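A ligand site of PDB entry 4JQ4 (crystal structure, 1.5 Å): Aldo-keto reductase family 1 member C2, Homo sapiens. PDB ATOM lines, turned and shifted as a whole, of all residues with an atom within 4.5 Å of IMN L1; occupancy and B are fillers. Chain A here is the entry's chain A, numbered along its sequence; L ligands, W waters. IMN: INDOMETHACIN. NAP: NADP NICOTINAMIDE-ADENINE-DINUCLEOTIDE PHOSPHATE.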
ATOM      1  N   TYR A  24     -13.742 -10.667  16.432  1.00  0.00           N
ATOM      2  CA  TYR A  24     -14.482  -9.387  16.404  1.00  0.00           C
ATOM      3  C   TYR A  24     -14.284  -8.652  17.738  1.00  0.00           C
ATOM      4  O   TYR A  24     -14.360  -9.265  18.748  1.00  0.00           O
ATOM      5  CB  TYR A  24     -15.986  -9.613  16.199  1.00  0.00           C
ATOM      6  CG  TYR A  24     -16.734  -8.258  16.243  1.00  0.00           C
ATOM      7  CD1 TYR A  24     -16.558  -7.344  15.222  1.00  0.00           C
ATOM      8  CD2 TYR A  24     -17.530  -7.883  17.364  1.00  0.00           C
ATOM      9  CE1 TYR A  24     -17.185  -6.088  15.260  1.00  0.00           C
ATOM     10  CE2 TYR A  24     -18.164  -6.628  17.424  1.00  0.00           C
ATOM     11  CZ  TYR A  24     -17.979  -5.741  16.357  1.00  0.00           C
ATOM     12  OH  TYR A  24     -18.557  -4.490  16.373  1.00  0.00           O
ATOM     13  N   VAL A  54     -16.453  -7.531   7.362  1.00  0.00           N
ATOM     14  CA  VAL A  54     -17.088  -6.383   8.057  1.00  0.00           C
ATOM     15  C   VAL A  54     -16.425  -6.089   9.365  1.00  0.00           C
ATOM     16  O   VAL A  54     -16.713  -5.080   9.926  1.00  0.00           O
ATOM     17  CB  VAL A  54     -18.606  -6.700   8.255  1.00  0.00           C
ATOM     18  CG1 VAL A  54     -18.792  -7.742   9.342  1.00  0.00           C
ATOM     19  CG2 VAL A  54     -19.435  -5.438   8.419  1.00  0.00           C
ATOM     20  N   TYR A  55     -15.600  -7.002   9.943  1.00  0.00           N
ATOM     21  CA  TYR A  55     -14.915  -6.801  11.233  1.00  0.00           C
ATOM     22  C   TYR A  55     -13.771  -5.767  11.111  1.00  0.00           C
ATOM     23  O   TYR A  55     -13.258  -5.256  12.118  1.00  0.00           O
ATOM     24  CB  TYR A  55     -14.311  -8.143  11.755  1.00  0.00           C
ATOM     25  CG  TYR A  55     -15.360  -9.200  12.065  1.00  0.00           C
ATOM     26  CD1 TYR A  55     -16.699  -8.960  12.028  1.00  0.00           C
ATOM     27  CD2 TYR A  55     -14.958 -10.517  12.436  1.00  0.00           C
ATOM     28  CE1 TYR A  55     -17.601  -9.984  12.296  1.00  0.00           C
ATOM     29  CE2 TYR A  55     -15.830 -11.519  12.649  1.00  0.00           C
ATOM     30  CZ  TYR A  55     -17.148 -11.283  12.618  1.00  0.00           C
ATOM     31  OH  TYR A  55     -17.985 -12.259  12.919  1.00  0.00           O
ATOM     32  N   HIS A 117     -22.673 -14.021   5.256  1.00  0.00           N
ATOM     33  CA  HIS A 117     -22.717 -13.485   6.602  1.00  0.00           C
ATOM     34  C   HIS A 117     -24.115 -13.253   7.212  1.00  0.00           C
ATOM     35  O   HIS A 117     -24.339 -13.519   8.318  1.00  0.00           O
ATOM     36  CB  HIS A 117     -21.815 -12.242   6.670  1.00  0.00           C
ATOM     37  CG  HIS A 117     -21.290 -11.924   8.039  1.00  0.00           C
ATOM     38  ND1 HIS A 117     -20.190 -11.220   8.217  1.00  0.00           N
ATOM     39  CD2 HIS A 117     -21.732 -12.254   9.285  1.00  0.00           C
ATOM     40  CE1 HIS A 117     -19.959 -11.093   9.493  1.00  0.00           C
ATOM     41  NE2 HIS A 117     -20.912 -11.713  10.154  1.00  0.00           N
ATOM     42  N   PHE A 118     -25.012 -12.704   6.426  1.00  0.00           N
ATOM     43  CA  PHE A 118     -26.296 -12.341   6.892  1.00  0.00           C
ATOM     44  C   PHE A 118     -27.201 -12.292   5.646  1.00  0.00           C
ATOM     45  O   PHE A 118     -26.789 -11.827   4.615  1.00  0.00           O
ATOM     46  CB  PHE A 118     -26.239 -11.021   7.687  1.00  0.00           C
ATOM     47  CG  PHE A 118     -27.456 -10.814   8.484  1.00  0.00           C
ATOM     48  CD1 PHE A 118     -27.521 -11.265   9.774  1.00  0.00           C
ATOM     49  CD2 PHE A 118     -28.532 -10.074   7.963  1.00  0.00           C
ATOM     50  CE1 PHE A 118     -28.630 -11.091  10.536  1.00  0.00           C
ATOM     51  CE2 PHE A 118     -29.672  -9.926   8.723  1.00  0.00           C
ATOM     52  CZ  PHE A 118     -29.737 -10.465   9.989  1.00  0.00           C
ATOM     53  N   VAL A 128     -20.142  -0.655   4.101  1.00  0.00           N
ATOM     54  CA  VAL A 128     -20.739  -1.853   4.637  1.00  0.00           C
ATOM     55  C   VAL A 128     -22.178  -1.687   5.155  1.00  0.00           C
ATOM     56  O   VAL A 128     -23.032  -2.616   4.942  1.00  0.00           O
ATOM     57  CB  VAL A 128     -19.847  -2.552   5.699  1.00  0.00           C
ATOM     58  CG1 VAL A 128     -18.529  -3.047   5.090  1.00  0.00           C
ATOM     59  CG2 VAL A 128     -19.579  -1.704   6.930  1.00  0.00           C
ATOM     60  N   ILE A 129     -22.529  -0.456   5.635  1.00  0.00           N
ATOM     61  CA  ILE A 129     -23.899  -0.123   6.021  1.00  0.00           C
ATOM     62  C   ILE A 129     -24.250   1.150   5.217  1.00  0.00           C
ATOM     63  O   ILE A 129     -24.173   2.275   5.721  1.00  0.00           O
ATOM     64  CB  ILE A 129     -24.056   0.139   7.517  1.00  0.00           C
ATOM     65  CG1 ILE A 129     -23.404  -0.990   8.366  1.00  0.00           C
ATOM     66  CG2 ILE A 129     -25.528   0.308   7.866  1.00  0.00           C
ATOM     67  CD1 ILE A 129     -24.198  -2.222   8.233  1.00  0.00           C
ATOM     68  N   ASN A 167     -26.390 -17.008  10.255  1.00  0.00           N
ATOM     69  CA  ASN A 167     -27.651 -16.396  10.541  1.00  0.00           C
ATOM     70  C   ASN A 167     -28.776 -16.807   9.627  1.00  0.00           C
ATOM     71  O   ASN A 167     -29.709 -15.970   9.349  1.00  0.00           O
ATOM     72  CB  ASN A 167     -27.485 -14.886  10.537  1.00  0.00           C
ATOM     73  CG  ASN A 167     -26.502 -14.437  11.564  1.00  0.00           C
ATOM     74  OD1 ASN A 167     -26.739 -14.622  12.793  1.00  0.00           O
ATOM     75  ND2 ASN A 167     -25.347 -13.909  11.124  1.00  0.00           N
ATOM     76  N   TYR A 216     -21.809 -18.851  17.761  1.00  0.00           N
ATOM     77  CA  TYR A 216     -21.236 -17.655  18.249  1.00  0.00           C
ATOM     78  C   TYR A 216     -21.936 -17.086  19.510  1.00  0.00           C
ATOM     79  O   TYR A 216     -23.052 -17.529  19.872  1.00  0.00           O
ATOM     80  CB  TYR A 216     -21.158 -16.656  17.132  1.00  0.00           C
ATOM     81  CG  TYR A 216     -22.415 -15.945  16.660  1.00  0.00           C
ATOM     82  CD1 TYR A 216     -23.072 -15.032  17.495  1.00  0.00           C
ATOM     83  CD2 TYR A 216     -22.965 -16.213  15.432  1.00  0.00           C
ATOM     84  CE1 TYR A 216     -24.131 -14.272  16.961  1.00  0.00           C
ATOM     85  CE2 TYR A 216     -24.018 -15.465  14.904  1.00  0.00           C
ATOM     86  CZ  TYR A 216     -24.626 -14.545  15.703  1.00  0.00           C
ATOM     87  OH  TYR A 216     -25.693 -13.794  15.161  1.00  0.00           O
ATOM     88  N   GLU A 224     -22.113  -5.456  23.385  1.00  0.00           N
ATOM     89  CA  GLU A 224     -21.762  -4.149  22.929  1.00  0.00           C
ATOM     90  C   GLU A 224     -23.050  -3.391  22.634  1.00  0.00           C
ATOM     91  O   GLU A 224     -23.913  -3.870  21.914  1.00  0.00           O
ATOM     92  CB  GLU A 224     -20.885  -4.280  21.698  1.00  0.00           C
ATOM     93  CG  GLU A 224     -20.388  -2.968  21.091  1.00  0.00           C
ATOM     94  CD  GLU A 224     -20.030  -3.132  19.630  1.00  0.00           C
ATOM     95  OE1 GLU A 224     -20.294  -4.251  19.045  1.00  0.00           O
ATOM     96  OE2 GLU A 224     -19.478  -2.150  19.086  1.00  0.00           O
ATOM     97  N   TRP A 227     -26.140  -2.851  20.155  1.00  0.00           N
ATOM     98  CA  TRP A 227     -26.524  -4.157  19.574  1.00  0.00           C
ATOM     99  C   TRP A 227     -27.090  -5.145  20.587  1.00  0.00           C
ATOM    100  O   TRP A 227     -27.914  -6.023  20.222  1.00  0.00           O
ATOM    101  CB  TRP A 227     -25.337  -4.781  18.832  1.00  0.00           C
ATOM    102  CG  TRP A 227     -24.724  -3.791  17.932  1.00  0.00           C
ATOM    103  CD1 TRP A 227     -23.512  -3.190  18.068  1.00  0.00           C
ATOM    104  CD2 TRP A 227     -25.359  -3.172  16.786  1.00  0.00           C
ATOM    105  NE1 TRP A 227     -23.314  -2.280  17.053  1.00  0.00           N
ATOM    106  CE2 TRP A 227     -24.423  -2.257  16.249  1.00  0.00           C
ATOM    107  CE3 TRP A 227     -26.587  -3.371  16.138  1.00  0.00           C
ATOM    108  CZ2 TRP A 227     -24.691  -1.518  15.103  1.00  0.00           C
ATOM    109  CZ3 TRP A 227     -26.860  -2.622  15.000  1.00  0.00           C
ATOM    110  CH2 TRP A 227     -25.914  -1.691  14.486  1.00  0.00           C
ATOM    111  N   LEU A 306     -28.386 -11.001  20.094  1.00  0.00           N
ATOM    112  CA  LEU A 306     -28.016 -10.287  18.877  1.00  0.00           C
ATOM    113  C   LEU A 306     -29.024 -10.423  17.706  1.00  0.00           C
ATOM    114  O   LEU A 306     -29.229 -11.483  17.148  1.00  0.00           O
ATOM    115  CB  LEU A 306     -26.651 -10.734  18.422  1.00  0.00           C
ATOM    116  CG  LEU A 306     -25.479 -10.340  19.326  1.00  0.00           C
ATOM    117  CD1 LEU A 306     -24.308 -11.197  18.894  1.00  0.00           C
ATOM    118  CD2 LEU A 306     -25.174  -8.846  19.289  1.00  0.00           C
ATOM    119  N   THR A 307     -29.639  -9.288  17.333  1.00  0.00           N
ATOM    120  CA  THR A 307     -30.718  -9.273  16.365  1.00  0.00           C
ATOM    121  C   THR A 307     -30.440  -8.487  15.072  1.00  0.00           C
ATOM    122  O   THR A 307     -31.188  -8.652  14.106  1.00  0.00           O
ATOM    123  CB  THR A 307     -31.980  -8.646  16.994  1.00  0.00           C
ATOM    124  OG1 THR A 307     -31.619  -7.382  17.515  1.00  0.00           O
ATOM    125  CG2 THR A 307     -32.543  -9.535  18.117  1.00  0.00           C
ATOM    126  N   LEU A 308     -29.388  -7.660  15.021  1.00  0.00           N
ATOM    127  CA  LEU A 308     -29.125  -6.802  13.836  1.00  0.00           C
ATOM    128  C   LEU A 308     -30.427  -6.137  13.282  1.00  0.00           C
ATOM    129  O   LEU A 308     -30.786  -6.286  12.106  1.00  0.00           O
ATOM    130  CB  LEU A 308     -28.453  -7.595  12.708  1.00  0.00           C
ATOM    131  CG  LEU A 308     -27.630  -6.755  11.682  1.00  0.00           C
ATOM    132  CD1 LEU A 308     -26.655  -5.769  12.255  1.00  0.00           C
ATOM    133  CD2 LEU A 308     -26.869  -7.656  10.683  1.00  0.00           C
ATOM    134  N   PHE A 319     -34.862 -13.533  11.810  1.00  0.00           N
ATOM    135  CA  PHE A 319     -35.368 -13.720  13.129  1.00  0.00           C
ATOM    136  C   PHE A 319     -36.825 -13.230  13.206  1.00  0.00           C
ATOM    137  O   PHE A 319     -37.290 -13.033  14.302  1.00  0.00           O
ATOM    138  CB  PHE A 319     -34.457 -13.025  14.148  1.00  0.00           C
ATOM    139  CG  PHE A 319     -32.982 -13.258  13.927  1.00  0.00           C
ATOM    140  CD1 PHE A 319     -32.460 -14.548  13.680  1.00  0.00           C
ATOM    141  CD2 PHE A 319     -32.090 -12.170  13.936  1.00  0.00           C
ATOM    142  CE1 PHE A 319     -31.090 -14.715  13.454  1.00  0.00           C
ATOM    143  CE2 PHE A 319     -30.747 -12.358  13.659  1.00  0.00           C
ATOM    144  CZ  PHE A 319     -30.243 -13.642  13.477  1.00  0.00           C
HETATM  145  C   IMN L   1     -23.606  -7.054  14.540  1.00  0.00           C
HETATM  146  C1  IMN L   1     -23.596  -8.308  13.986  1.00  0.00           C
HETATM  147  C2  IMN L   1     -24.596  -9.201  14.213  1.00  0.00           C
HETATM  148  C3  IMN L   1     -25.686  -8.812  15.027  1.00  0.00           C
HETATM  149  C4  IMN L   1     -25.683  -7.519  15.578  1.00  0.00           C
HETATM  150  C5  IMN L   1     -24.616  -6.644  15.334  1.00  0.00           C
HETATM  151  C6  IMN L   1     -26.997 -10.668  14.303  1.00  0.00           C
HETATM  152  C7  IMN L   1     -22.456  -8.369  13.263  1.00  0.00           C
HETATM  153  C8  IMN L   1     -21.782  -7.215  13.340  1.00  0.00           C
HETATM  154  C9  IMN L   1     -22.179  -5.103  14.490  1.00  0.00           C
HETATM  155  C10 IMN L   1     -21.662  -4.260  13.477  1.00  0.00           C
HETATM  156  C11 IMN L   1     -20.625  -3.381  13.824  1.00  0.00           C
HETATM  157  C12 IMN L   1     -20.033  -2.575  12.869  1.00  0.00           C
HETATM  158  C13 IMN L   1     -20.434  -2.631  11.540  1.00  0.00           C
HETATM  159  C14 IMN L   1     -21.459  -3.517  11.149  1.00  0.00           C
HETATM  160  C15 IMN L   1     -22.061  -4.343  12.109  1.00  0.00           C
HETATM  161  C16 IMN L   1     -20.370  -6.935  12.670  1.00  0.00           C
HETATM  162  C17 IMN L   1     -21.948  -9.578  12.463  1.00  0.00           C
HETATM  163  C18 IMN L   1     -20.837 -10.348  13.308  1.00  0.00           C
HETATM  164  N   IMN L   1     -22.487  -6.384  14.145  1.00  0.00           N
HETATM  165  O   IMN L   1     -26.789  -9.596  15.317  1.00  0.00           O
HETATM  166  O1  IMN L   1     -22.205  -4.757  15.680  1.00  0.00           O
HETATM  167  O2  IMN L   1     -20.361 -11.344  12.745  1.00  0.00           O
HETATM  168  O3  IMN L   1     -20.505  -9.938  14.463  1.00  0.00           O
HETATM  169 CL   IMN L   1     -19.600  -1.536  10.391  1.00  0.00          CL
HETATM  170  PA  NAP L   2     -18.140 -14.418  22.975  1.00  0.00           P
HETATM  171  O1A NAP L   2     -19.440 -14.800  23.589  1.00  0.00           O
HETATM  172  O2A NAP L   2     -17.110 -15.491  22.665  1.00  0.00           O
HETATM  173  O5B NAP L   2     -17.304 -13.694  24.212  1.00  0.00           O
HETATM  174  C5B NAP L   2     -17.883 -12.726  24.994  1.00  0.00           C
HETATM  175  C4B NAP L   2     -16.933 -12.162  26.042  1.00  0.00           C
HETATM  176  O4B NAP L   2     -16.385 -13.124  26.896  1.00  0.00           O
HETATM  177  C3B NAP L   2     -15.705 -11.516  25.336  1.00  0.00           C
HETATM  178  O3B NAP L   2     -15.883 -10.243  25.262  1.00  0.00           O
HETATM  179  C2B NAP L   2     -14.533 -11.862  26.225  1.00  0.00           C
HETATM  180  O2B NAP L   2     -13.795 -10.782  26.819  1.00  0.00           O
HETATM  181  C1B NAP L   2     -15.148 -12.672  27.351  1.00  0.00           C
HETATM  182  N9A NAP L   2     -14.410 -13.931  27.665  1.00  0.00           N
HETATM  183  C8A NAP L   2     -13.773 -14.778  26.810  1.00  0.00           C
HETATM  184  N7A NAP L   2     -13.272 -15.825  27.471  1.00  0.00           N
HETATM  185  C5A NAP L   2     -13.591 -15.651  28.776  1.00  0.00           C
HETATM  186  C6A NAP L   2     -13.336 -16.414  29.884  1.00  0.00           C
HETATM  187  N6A NAP L   2     -12.603 -17.568  29.791  1.00  0.00           N
HETATM  188  N1A NAP L   2     -13.801 -16.048  31.112  1.00  0.00           N
HETATM  189  C2A NAP L   2     -14.529 -14.862  31.195  1.00  0.00           C
HETATM  190  N3A NAP L   2     -14.815 -14.051  30.056  1.00  0.00           N
HETATM  191  C4A NAP L   2     -14.332 -14.505  28.861  1.00  0.00           C
HETATM  192  O3  NAP L   2     -18.144 -13.045  22.098  1.00  0.00           O
HETATM  193  PN  NAP L   2     -18.611 -12.715  20.570  1.00  0.00           P
HETATM  194  O1N NAP L   2     -19.975 -12.280  20.654  1.00  0.00           O
HETATM  195  O2N NAP L   2     -17.417 -11.859  20.335  1.00  0.00           O
HETATM  196  O5D NAP L   2     -18.662 -14.084  19.741  1.00  0.00           O
HETATM  197  C5D NAP L   2     -17.389 -14.717  19.452  1.00  0.00           C
HETATM  198  C4D NAP L   2     -17.095 -14.627  17.991  1.00  0.00           C
HETATM  199  O4D NAP L   2     -18.252 -15.235  17.164  1.00  0.00           O
HETATM  200  C3D NAP L   2     -16.876 -13.165  17.405  1.00  0.00           C
HETATM  201  O3D NAP L   2     -15.647 -12.640  17.753  1.00  0.00           O
HETATM  202  C2D NAP L   2     -16.966 -13.501  15.884  1.00  0.00           C
HETATM  203  O2D NAP L   2     -15.748 -14.168  15.408  1.00  0.00           O
HETATM  204  C1D NAP L   2     -18.229 -14.482  15.864  1.00  0.00           C
HETATM  205  N1N NAP L   2     -19.517 -13.796  15.668  1.00  0.00           N
HETATM  206  C2N NAP L   2     -20.202 -14.084  14.532  1.00  0.00           C
HETATM  207  C3N NAP L   2     -21.423 -13.460  14.250  1.00  0.00           C
HETATM  208  C7N NAP L   2     -22.136 -13.676  13.044  1.00  0.00           C
HETATM  209  O7N NAP L   2     -23.136 -12.944  12.691  1.00  0.00           O
HETATM  210  N7N NAP L   2     -21.689 -14.675  12.260  1.00  0.00           N
HETATM  211  C4N NAP L   2     -21.944 -12.638  15.286  1.00  0.00           C
HETATM  212  C5N NAP L   2     -21.288 -12.370  16.463  1.00  0.00           C
HETATM  213  C6N NAP L   2     -20.087 -13.019  16.714  1.00  0.00           C
HETATM  214  P2B NAP L   2     -12.226 -10.673  26.882  1.00  0.00           P
HETATM  215  O1X NAP L   2     -11.896 -10.438  25.437  1.00  0.00           O
HETATM  216  O2X NAP L   2     -11.849  -9.526  27.725  1.00  0.00           O
HETATM  217  O3X NAP L   2     -11.701 -11.975  27.424  1.00  0.00           O
HETATM  218  O   HOH W   1     -21.566  -8.444  16.810  1.00  0.00           O
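Tyr 24 touches IMN L1.
Val 54 touches IMN L1 (CG1 to C16, 3.8 Å).
Val 128 touches IMN L1 (CG2 to CL, 3.5 Å).
Tyr 216 touches IMN L1.
Glu 224 touches IMN L1.
CB of Leu 306 touches O of IMN L1 (3.3 Å).
Thr 307 touches IMN L1 (N to O, 3.5 Å).
Hydrophobic or aromatic side chains within 4 Å of IMN L1: Val 54, Tyr 55, His 117, Val 128, Trp 227, Leu 306 and Leu 308.
Within 4 Å of IMN L1: Tyr 24, Val 54, Tyr 55, His 117, Val 128, Tyr 216, Glu 224, Trp 227, Leu 306, Thr 307 and Leu 308.
The backbone carbonyl oxygen (O) of His 117 is in hydrogen-bond range of the side-chain amide nitrogen (ND2) of Asn 167 (3.0 Å).
The side-chain hydroxyl (OH) of Tyr 216 lies within hydrogen-bond range of the side-chain amide oxygen (OD1) of Asn 167 (2.7 Å).
The side-chain hydroxyl (OH) of Tyr 24 is in hydrogen-bond range of the side-chain carboxylate (OE1) of Glu 224 (3.2 Å).
The indole nitrogen of Trp 227 sits at hydrogen-bond distance from an oxygen (O1) of IMN L1.
N of Leu 308 is in hydrogen-bond range of O of IMN L1 (3.3 Å).
An oxygen (O3D) of NAP L2 sits at hydrogen-bond distance from the backbone NH (N) of Tyr 24, at 3.0 Å.
The side-chain hydroxyl (OH) of Tyr 55 is in hydrogen-bond range of an oxygen (O2) of IMN L1.
An oxygen (O2) of IMN L1 lies within hydrogen-bond range of a ring nitrogen (NE2) of His 117.
O7N of NAP L2 is in hydrogen-bond range of ND2 of Asn 167 (2.9 Å).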
